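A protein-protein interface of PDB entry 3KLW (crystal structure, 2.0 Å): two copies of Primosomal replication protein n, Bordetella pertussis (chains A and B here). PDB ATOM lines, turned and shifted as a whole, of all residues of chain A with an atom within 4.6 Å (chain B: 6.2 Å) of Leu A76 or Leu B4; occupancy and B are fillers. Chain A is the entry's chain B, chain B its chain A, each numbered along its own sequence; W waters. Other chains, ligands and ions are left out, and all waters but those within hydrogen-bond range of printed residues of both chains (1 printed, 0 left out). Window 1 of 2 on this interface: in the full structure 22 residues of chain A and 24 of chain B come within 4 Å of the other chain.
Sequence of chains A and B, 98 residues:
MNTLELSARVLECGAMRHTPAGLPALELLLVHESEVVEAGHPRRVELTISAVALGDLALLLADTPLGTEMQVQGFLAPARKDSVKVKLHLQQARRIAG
N of Glu B5 is in hydrogen-bond range of O of Thr A3, at 2.9 Å.
Of the printed residues of chain B, Thr A3 touches Thr B3 (3.7 Å), Leu B4 (3.5 Å) and Glu B5 (2.9 Å).
Printed residues of chain A within 4 Å of His B32: Asn A2.
Of the printed residues of chain B, Ala A77 touches Arg B43 (3.6 Å).
Printed residues of chain B within 4 Å of Asn A2: Glu B5 (3.5 Å), Leu B6 (3.9 Å), His B32 (3.6 Å) and Val B45 (3.7 Å).
Gln B73 touches none of the printed residues of chain A.
The nearest residue of chain A that does not touch Leu B4 is Asn A2 (4.3 Å).
The nearest printed residue of chain A that does not touch His B32 is Leu A76 (5.6 Å).
Thr A3 touches its own counterpart, Thr B3.
Thr A3 touches Leu B4, and with the chains exchanged Leu A4 touches Thr B3.
Leu B4 touches its own counterpart, Leu A4.
Leu A4 touches Leu B76, and with the chains exchanged Leu A76 touches Leu B4.
Positions printed for both chains: 2, 3, 4, 74, 75, 76, 86 and 88.
Of the 19 pairs that touch across the chains among the printed residues, 8 have their exchanged pair printed and touching as well.
The side-chain amide nitrogen (ND2) of Asn B2 is in hydrogen-bond range of the backbone carbonyl oxygen (O) of Leu B76 (2.9 Å).
The backbone carbonyl oxygen (O) of Gly B74 lies within hydrogen-bond range of the backbone NH (N) of Leu B4 (2.7 Å).
The backbone NH of His B32 is in hydrogen-bond range of the backbone carbonyl oxygen of Leu B47 (2.7 Å).
The side-chain amide nitrogen of Asn A2 is in hydrogen-bond range of the backbone carbonyl oxygen of Leu A76, 2.8 Å away.
The backbone NH (N) of Leu A4 lies within hydrogen-bond range of the backbone carbonyl oxygen (O) of Gly A74, at 2.9 Å.
O of Ala A77 lies within hydrogen-bond range of N of Lys A87 (2.8 Å).
Among the printed residues, pairs that only touch across the chains: Asn A2 with Glu B5 (3.5 Å), Asn A2 with Leu B6 (3.9 Å), Asn A2 with His B32 (3.6 Å), Asn A2 with Val B45 (3.7 Å), Thr A3 with Thr B3 (3.7 Å), Thr A3 with Leu B4 (3.5 Å), Leu A4 with Thr B3 (3.4 Å), Leu A4 with Leu B4 (3.9 Å), Leu A4 with Leu B76 (3.6 Å), Phe A75 with Arg B43 (3.8 Å), Phe A75 with Val B45 (3.7 Å), Leu A76 with Leu B4 (3.97 Å), Leu A76 with Val B45 (3.6 Å), Leu A76 with Leu B47 (3.9 Å), Leu A76 with Leu B76 (3.96 Å), Ala A77 with Arg B43 (3.6 Å), Val A86 with Leu B47 (3.9 Å) and Val A86 with Val B86 (3.6 Å).
Water W1 lies within hydrogen-bond range of the backbone carbonyl oxygen (O) of Thr A3 (2.9 Å) and the backbone carbonyl oxygen (O) of Thr B3 (3.0 Å).
Printed residues of chain A that touch a printed residue of chain B: Asn A2, Thr A3, Leu A4, Phe A75, Leu A76, Ala A77 and Val A86.
Hydrophobic or aromatic side chains of chain A within 4 Å of the printed part of chain B: Leu A4, Phe A75, Leu A76, Ala A77 and Val A86.
Printed residues of chain B that touch a printed residue of chain A: Thr B3, Leu B4, Glu B5, Leu B6, His B32, Arg B43, Val B45, Leu B47, Leu B76 and Val B86.
Hydrophobic or aromatic side chains of chain B that line the printed part of chain A: Leu B4, Leu B6, His B32, Val B45, Leu B47, Leu B76 and Val B86.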
ATOM      1  N   ASN A   2      25.430  15.971  26.334  1.00  0.00           N
ATOM      2  CA  ASN A   2      25.173  14.648  25.748  1.00  0.00           C
ATOM      3  C   ASN A   2      24.749  13.736  26.911  1.00  0.00           C
ATOM      4  O   ASN A   2      25.576  13.117  27.560  1.00  0.00           O
ATOM      5  CB  ASN A   2      26.462  14.135  25.073  1.00  0.00           C
ATOM      6  CG  ASN A   2      26.299  12.749  24.430  1.00  0.00           C
ATOM      7  OD1 ASN A   2      25.294  12.064  24.618  1.00  0.00           O
ATOM      8  ND2 ASN A   2      27.291  12.346  23.669  1.00  0.00           N
ATOM      9  N   THR A   3      23.457  13.669  27.202  1.00  0.00           N
ATOM     10  CA  THR A   3      23.000  12.857  28.317  1.00  0.00           C
ATOM     11  C   THR A   3      21.685  12.183  28.015  1.00  0.00           C
ATOM     12  O   THR A   3      20.712  12.858  27.717  1.00  0.00           O
ATOM     13  CB  THR A   3      22.750  13.696  29.608  1.00  0.00           C
ATOM     14  OG1 THR A   3      23.999  14.175  30.108  1.00  0.00           O
ATOM     15  CG2 THR A   3      22.127  12.830  30.683  1.00  0.00           C
ATOM     16  N   LEU A   4      21.673  10.862  28.148  1.00  0.00           N
ATOM     17  CA  LEU A   4      20.503  10.035  27.941  1.00  0.00           C
ATOM     18  C   LEU A   4      20.071   9.405  29.267  1.00  0.00           C
ATOM     19  O   LEU A   4      20.915   8.833  29.974  1.00  0.00           O
ATOM     20  CB  LEU A   4      20.798   8.901  26.954  1.00  0.00           C
ATOM     21  CG  LEU A   4      19.678   7.846  26.840  1.00  0.00           C
ATOM     22  CD1 LEU A   4      18.479   8.426  26.052  1.00  0.00           C
ATOM     23  CD2 LEU A   4      20.206   6.637  26.066  1.00  0.00           C
ATOM     24  N   GLY A  74      23.783   8.237  31.040  1.00  0.00           N
ATOM     25  CA  GLY A  74      25.134   8.347  30.506  1.00  0.00           C
ATOM     26  C   GLY A  74      25.186   9.087  29.173  1.00  0.00           C
ATOM     27  O   GLY A  74      24.217   9.750  28.802  1.00  0.00           O
ATOM     28  N   PHE A  75      26.305   9.011  28.455  1.00  0.00           N
ATOM     29  CA  PHE A  75      26.391   9.696  27.182  1.00  0.00           C
ATOM     30  C   PHE A  75      26.434   8.683  25.997  1.00  0.00           C
ATOM     31  O   PHE A  75      26.864   7.505  26.157  1.00  0.00           O
ATOM     32  CB  PHE A  75      27.622  10.612  27.156  1.00  0.00           C
ATOM     33  CG  PHE A  75      28.946   9.861  27.243  1.00  0.00           C
ATOM     34  CD1 PHE A  75      29.556   9.377  26.111  1.00  0.00           C
ATOM     35  CD2 PHE A  75      29.579   9.670  28.483  1.00  0.00           C
ATOM     36  CE1 PHE A  75      30.799   8.670  26.195  1.00  0.00           C
ATOM     37  CE2 PHE A  75      30.796   8.980  28.582  1.00  0.00           C
ATOM     38  CZ  PHE A  75      31.412   8.488  27.431  1.00  0.00           C
ATOM     39  N   LEU A  76      25.972   9.140  24.830  1.00  0.00           N
ATOM     40  CA  LEU A  76      25.964   8.310  23.627  1.00  0.00           C
ATOM     41  C   LEU A  76      27.182   8.609  22.765  1.00  0.00           C
ATOM     42  O   LEU A  76      27.602   9.772  22.644  1.00  0.00           O
ATOM     43  CB  LEU A  76      24.720   8.584  22.790  1.00  0.00           C
ATOM     44  CG  LEU A  76      23.346   8.126  23.258  1.00  0.00           C
ATOM     45  CD1 LEU A  76      22.324   8.637  22.227  1.00  0.00           C
ATOM     46  CD2 LEU A  76      23.255   6.593  23.352  1.00  0.00           C
ATOM     47  N   ALA A  77      27.734   7.560  22.166  1.00  0.00           N
ATOM     48  CA  ALA A  77      28.902   7.690  21.302  1.00  0.00           C
ATOM     49  C   ALA A  77      28.811   6.592  20.264  1.00  0.00           C
ATOM     50  O   ALA A  77      28.157   5.568  20.486  1.00  0.00           O
ATOM     51  CB  ALA A  77      30.255   7.563  22.123  1.00  0.00           C
ATOM     52  N   VAL A  86      25.265   3.067  17.742  1.00  0.00           N
ATOM     53  CA  VAL A  86      25.611   3.835  18.939  1.00  0.00           C
ATOM     54  C   VAL A  86      25.717   2.957  20.170  1.00  0.00           C
ATOM     55  O   VAL A  86      25.231   1.839  20.178  1.00  0.00           O
ATOM     56  CB  VAL A  86      24.581   4.967  19.249  1.00  0.00           C
ATOM     57  CG1 VAL A  86      24.579   5.958  18.149  1.00  0.00           C
ATOM     58  CG2 VAL A  86      23.196   4.415  19.452  1.00  0.00           C
ATOM     59  N   LYS A  87      26.404   3.464  21.184  1.00  0.00           N
ATOM     60  CA  LYS A  87      26.517   2.772  22.458  1.00  0.00           C
ATOM     61  C   LYS A  87      26.272   3.802  23.548  1.00  0.00           C
ATOM     62  O   LYS A  87      26.689   4.958  23.422  1.00  0.00           O
ATOM     63  CB  LYS A  87      27.900   2.164  22.698  1.00  0.00           C
ATOM     64  CG  LYS A  87      28.122   0.815  22.057  1.00  0.00           C
ATOM     65  CD  LYS A  87      29.336   0.102  22.616  1.00  0.00           C
ATOM     66  CE  LYS A  87      29.705  -1.096  21.746  1.00  0.00           C
ATOM     67  NZ  LYS A  87      28.469  -1.853  21.381  1.00  0.00           N
ATOM     68  N   LEU A  88      25.568   3.379  24.595  1.00  0.00           N
ATOM     69  CA  LEU A  88      25.325   4.213  25.747  1.00  0.00           C
ATOM     70  C   LEU A  88      26.479   3.909  26.727  1.00  0.00           C
ATOM     71  O   LEU A  88      26.632   2.752  27.158  1.00  0.00           O
ATOM     72  CB  LEU A  88      24.004   3.824  26.384  1.00  0.00           C
ATOM     73  CG  LEU A  88      23.782   4.453  27.756  1.00  0.00           C
ATOM     74  CD1 LEU A  88      23.964   6.007  27.620  1.00  0.00           C
ATOM     75  CD2 LEU A  88      22.365   4.076  28.286  1.00  0.00           C
ATOM     76  N   ASN B   2      12.837   7.893  28.913  1.00  0.00           N
ATOM     77  CA  ASN B   2      13.552   7.848  27.631  1.00  0.00           C
ATOM     78  C   ASN B   2      13.746   9.285  27.146  1.00  0.00           C
ATOM     79  O   ASN B   2      12.937   9.790  26.409  1.00  0.00           O
ATOM     80  CB  ASN B   2      12.721   7.052  26.625  1.00  0.00           C
ATOM     81  CG  ASN B   2      13.366   6.962  25.246  1.00  0.00           C
ATOM     82  OD1 ASN B   2      14.439   7.509  24.977  1.00  0.00           O
ATOM     83  ND2 ASN B   2      12.710   6.237  24.368  1.00  0.00           N
ATOM     84  N   THR B   3      14.818   9.930  27.561  1.00  0.00           N
ATOM     85  CA  THR B   3      15.051  11.319  27.190  1.00  0.00           C
ATOM     86  C   THR B   3      16.504  11.609  26.954  1.00  0.00           C
ATOM     87  O   THR B   3      17.352  11.411  27.826  1.00  0.00           O
ATOM     88  CB  THR B   3      14.519  12.321  28.280  1.00  0.00           C
ATOM     89  OG1 THR B   3      14.873  13.676  27.914  1.00  0.00           O
ATOM     90  CG2 THR B   3      15.179  12.043  29.654  1.00  0.00           C
ATOM     91  N   LEU B   4      16.798  12.048  25.742  1.00  0.00           N
ATOM     92  CA  LEU B   4      18.147  12.427  25.392  1.00  0.00           C
ATOM     93  C   LEU B   4      18.240  13.952  25.309  1.00  0.00           C
ATOM     94  O   LEU B   4      17.393  14.579  24.691  1.00  0.00           O
ATOM     95  CB  LEU B   4      18.529  11.888  24.029  1.00  0.00           C
ATOM     96  CG  LEU B   4      19.878  12.399  23.489  1.00  0.00           C
ATOM     97  CD1 LEU B   4      21.031  11.754  24.321  1.00  0.00           C
ATOM     98  CD2 LEU B   4      20.073  11.978  22.014  1.00  0.00           C
ATOM     99  N   GLU B   5      19.246  14.555  25.928  1.00  0.00           N
ATOM    100  CA  GLU B   5      19.451  15.998  25.779  1.00  0.00           C
ATOM    101  C   GLU B   5      20.774  16.100  25.064  1.00  0.00           C
ATOM    102  O   GLU B   5      21.744  15.474  25.459  1.00  0.00           O
ATOM    103  CB  GLU B   5      19.562  16.687  27.123  1.00  0.00           C
ATOM    104  CG  GLU B   5      18.232  17.082  27.666  1.00  0.00           C
ATOM    105  CD  GLU B   5      18.388  17.664  29.031  1.00  0.00           C
ATOM    106  OE1 GLU B   5      19.471  18.278  29.259  1.00  0.00           O
ATOM    107  OE2 GLU B   5      17.439  17.512  29.847  1.00  0.00           O
ATOM    108  N   LEU B   6      20.825  16.882  24.003  1.00  0.00           N
ATOM    109  CA  LEU B   6      22.048  16.998  23.252  1.00  0.00           C
ATOM    110  C   LEU B   6      22.268  18.377  22.637  1.00  0.00           C
ATOM    111  O   LEU B   6      21.301  19.026  22.219  1.00  0.00           O
ATOM    112  CB  LEU B   6      22.016  15.958  22.136  1.00  0.00           C
ATOM    113  CG  LEU B   6      23.211  15.704  21.225  1.00  0.00           C
ATOM    114  CD1 LEU B   6      24.214  14.830  21.943  1.00  0.00           C
ATOM    115  CD2 LEU B   6      22.706  14.988  19.938  1.00  0.00           C
ATOM    116  N   HIS B  32      27.299  16.138  17.049  1.00  0.00           N
ATOM    117  CA  HIS B  32      27.677  16.553  18.394  1.00  0.00           C
ATOM    118  C   HIS B  32      29.165  16.345  18.627  1.00  0.00           C
ATOM    119  O   HIS B  32      29.724  15.340  18.190  1.00  0.00           O
ATOM    120  CB  HIS B  32      26.945  15.720  19.437  1.00  0.00           C
ATOM    121  CG  HIS B  32      27.439  15.935  20.827  1.00  0.00           C
ATOM    122  ND1 HIS B  32      28.410  15.144  21.409  1.00  0.00           N
ATOM    123  CD2 HIS B  32      27.112  16.869  21.754  1.00  0.00           C
ATOM    124  CE1 HIS B  32      28.655  15.574  22.635  1.00  0.00           C
ATOM    125  NE2 HIS B  32      27.879  16.620  22.866  1.00  0.00           N
ATOM    126  N   ARG B  43      37.939  11.845  27.302  1.00  0.00           N
ATOM    127  CA  ARG B  43      37.549  11.147  26.072  1.00  0.00           C
ATOM    128  C   ARG B  43      36.800  12.060  25.094  1.00  0.00           C
ATOM    129  O   ARG B  43      35.851  12.752  25.459  1.00  0.00           O
ATOM    130  CB  ARG B  43      36.671   9.939  26.416  1.00  0.00           C
ATOM    131  CG  ARG B  43      36.279   9.070  25.231  1.00  0.00           C
ATOM    132  CD  ARG B  43      35.335   7.944  25.662  1.00  0.00           C
ATOM    133  NE  ARG B  43      35.028   7.001  24.585  1.00  0.00           N
ATOM    134  CZ  ARG B  43      34.156   7.217  23.599  1.00  0.00           C
ATOM    135  NH1 ARG B  43      33.481   8.360  23.532  1.00  0.00           N
ATOM    136  NH2 ARG B  43      33.954   6.286  22.672  1.00  0.00           N
ATOM    137  N   VAL B  45      34.253  12.820  22.225  1.00  0.00           N
ATOM    138  CA  VAL B  45      33.048  12.168  21.727  1.00  0.00           C
ATOM    139  C   VAL B  45      32.535  12.962  20.533  1.00  0.00           C
ATOM    140  O   VAL B  45      32.312  14.160  20.651  1.00  0.00           O
ATOM    141  CB  VAL B  45      31.912  12.111  22.780  1.00  0.00           C
ATOM    142  CG1 VAL B  45      30.620  11.627  22.110  1.00  0.00           C
ATOM    143  CG2 VAL B  45      32.280  11.178  23.928  1.00  0.00           C
ATOM    144  N   LEU B  47      29.482  12.465  17.814  1.00  0.00           N
ATOM    145  CA  LEU B  47      28.277  11.681  17.492  1.00  0.00           C
ATOM    146  C   LEU B  47      27.469  12.309  16.352  1.00  0.00           C
ATOM    147  O   LEU B  47      27.200  13.488  16.388  1.00  0.00           O
ATOM    148  CB  LEU B  47      27.370  11.628  18.742  1.00  0.00           C
ATOM    149  CG  LEU B  47      25.989  10.933  18.694  1.00  0.00           C
ATOM    150  CD1 LEU B  47      26.217   9.474  18.555  1.00  0.00           C
ATOM    151  CD2 LEU B  47      25.142  11.198  19.979  1.00  0.00           C
ATOM    152  N   ILE B  49      23.844  11.984  14.518  1.00  0.00           N
ATOM    153  CA  ILE B  49      22.593  11.276  14.732  1.00  0.00           C
ATOM    154  C   ILE B  49      21.460  11.879  13.915  1.00  0.00           C
ATOM    155  O   ILE B  49      21.365  13.099  13.753  1.00  0.00           O
ATOM    156  CB  ILE B  49      22.229  11.263  16.241  1.00  0.00           C
ATOM    157  CG1 ILE B  49      20.835  10.664  16.491  1.00  0.00           C
ATOM    158  CG2 ILE B  49      22.187  12.677  16.798  1.00  0.00           C
ATOM    159  CD1 ILE B  49      20.695   9.223  16.245  1.00  0.00           C
ATOM    160  N   VAL B  72      18.844  20.389  21.730  1.00  0.00           N
ATOM    161  CA  VAL B  72      17.609  19.660  21.595  1.00  0.00           C
ATOM    162  C   VAL B  72      17.441  18.646  22.688  1.00  0.00           C
ATOM    163  O   VAL B  72      18.412  18.318  23.423  1.00  0.00           O
ATOM    164  CB  VAL B  72      17.566  18.891  20.273  1.00  0.00           C
ATOM    165  CG1 VAL B  72      17.651  19.876  19.073  1.00  0.00           C
ATOM    166  CG2 VAL B  72      18.743  17.863  20.217  1.00  0.00           C
ATOM    167  N   GLN B  73      16.218  18.131  22.778  1.00  0.00           N
ATOM    168  CA  GLN B  73      15.895  17.057  23.714  1.00  0.00           C
ATOM    169  C   GLN B  73      14.722  16.303  23.104  1.00  0.00           C
ATOM    170  O   GLN B  73      13.903  16.862  22.348  1.00  0.00           O
ATOM    171  CB  GLN B  73      15.554  17.610  25.112  1.00  0.00           C
ATOM    172  CG  GLN B  73      14.126  17.922  25.398  1.00  0.00           C
ATOM    173  CD  GLN B  73      13.236  16.695  25.608  1.00  0.00           C
ATOM    174  OE1 GLN B  73      13.649  15.657  26.119  1.00  0.00           O
ATOM    175  NE2 GLN B  73      11.994  16.845  25.256  1.00  0.00           N
ATOM    176  N   GLY B  74      14.678  15.006  23.370  1.00  0.00           N
ATOM    177  CA  GLY B  74      13.605  14.210  22.838  1.00  0.00           C
ATOM    178  C   GLY B  74      13.840  12.773  23.227  1.00  0.00           C
ATOM    179  O   GLY B  74      14.679  12.511  24.063  1.00  0.00           O
ATOM    180  N   PHE B  75      13.105  11.846  22.626  1.00  0.00           N
ATOM    181  CA  PHE B  75      13.288  10.444  22.944  1.00  0.00           C
ATOM    182  C   PHE B  75      13.870   9.664  21.772  1.00  0.00           C
ATOM    183  O   PHE B  75      13.718  10.045  20.594  1.00  0.00           O
ATOM    184  CB  PHE B  75      11.951   9.828  23.398  1.00  0.00           C
ATOM    185  CG  PHE B  75      10.870   9.849  22.349  1.00  0.00           C
ATOM    186  CD1 PHE B  75      10.691   8.753  21.481  1.00  0.00           C
ATOM    187  CD2 PHE B  75      10.044  10.973  22.218  1.00  0.00           C
ATOM    188  CE1 PHE B  75       9.680   8.777  20.466  1.00  0.00           C
ATOM    189  CE2 PHE B  75       9.051  11.024  21.233  1.00  0.00           C
ATOM    190  CZ  PHE B  75       8.871   9.916  20.348  1.00  0.00           C
ATOM    191  N   LEU B  76      14.551   8.578  22.114  1.00  0.00           N
ATOM    192  CA  LEU B  76      15.172   7.693  21.135  1.00  0.00           C
ATOM    193  C   LEU B  76      14.191   6.615  20.700  1.00  0.00           C
ATOM    194  O   LEU B  76      13.437   6.102  21.526  1.00  0.00           O
ATOM    195  CB  LEU B  76      16.405   6.999  21.745  1.00  0.00           C
ATOM    196  CG  LEU B  76      17.601   7.903  22.100  1.00  0.00           C
ATOM    197  CD1 LEU B  76      18.725   7.057  22.691  1.00  0.00           C
ATOM    198  CD2 LEU B  76      18.086   8.626  20.811  1.00  0.00           C
ATOM    199  N   VAL B  86      19.331   3.905  15.718  1.00  0.00           N
ATOM    200  CA  VAL B  86      18.440   4.762  16.488  1.00  0.00           C
ATOM    201  C   VAL B  86      18.336   6.194  15.974  1.00  0.00           C
ATOM    202  O   VAL B  86      19.313   6.767  15.468  1.00  0.00           O
ATOM    203  CB  VAL B  86      18.862   4.793  17.978  1.00  0.00           C
ATOM    204  CG1 VAL B  86      19.165   3.361  18.462  1.00  0.00           C
ATOM    205  CG2 VAL B  86      20.066   5.635  18.145  1.00  0.00           C
ATOM    206  N   LEU B  88      16.685  10.195  16.953  1.00  0.00           N
ATOM    207  CA  LEU B  88      16.167  11.042  17.986  1.00  0.00           C
ATOM    208  C   LEU B  88      14.834  11.720  17.553  1.00  0.00           C
ATOM    209  O   LEU B  88      14.801  12.419  16.558  1.00  0.00           O
ATOM    210  CB  LEU B  88      17.205  12.099  18.323  1.00  0.00           C
ATOM    211  CG  LEU B  88      16.718  13.243  19.213  1.00  0.00           C
ATOM    212  CD1 LEU B  88      16.347  12.696  20.596  1.00  0.00           C
ATOM    213  CD2 LEU B  88      17.824  14.369  19.287  1.00  0.00           C
HETATM  214  O   HOH W   1      18.560  13.547  29.466  1.00  0.00           O
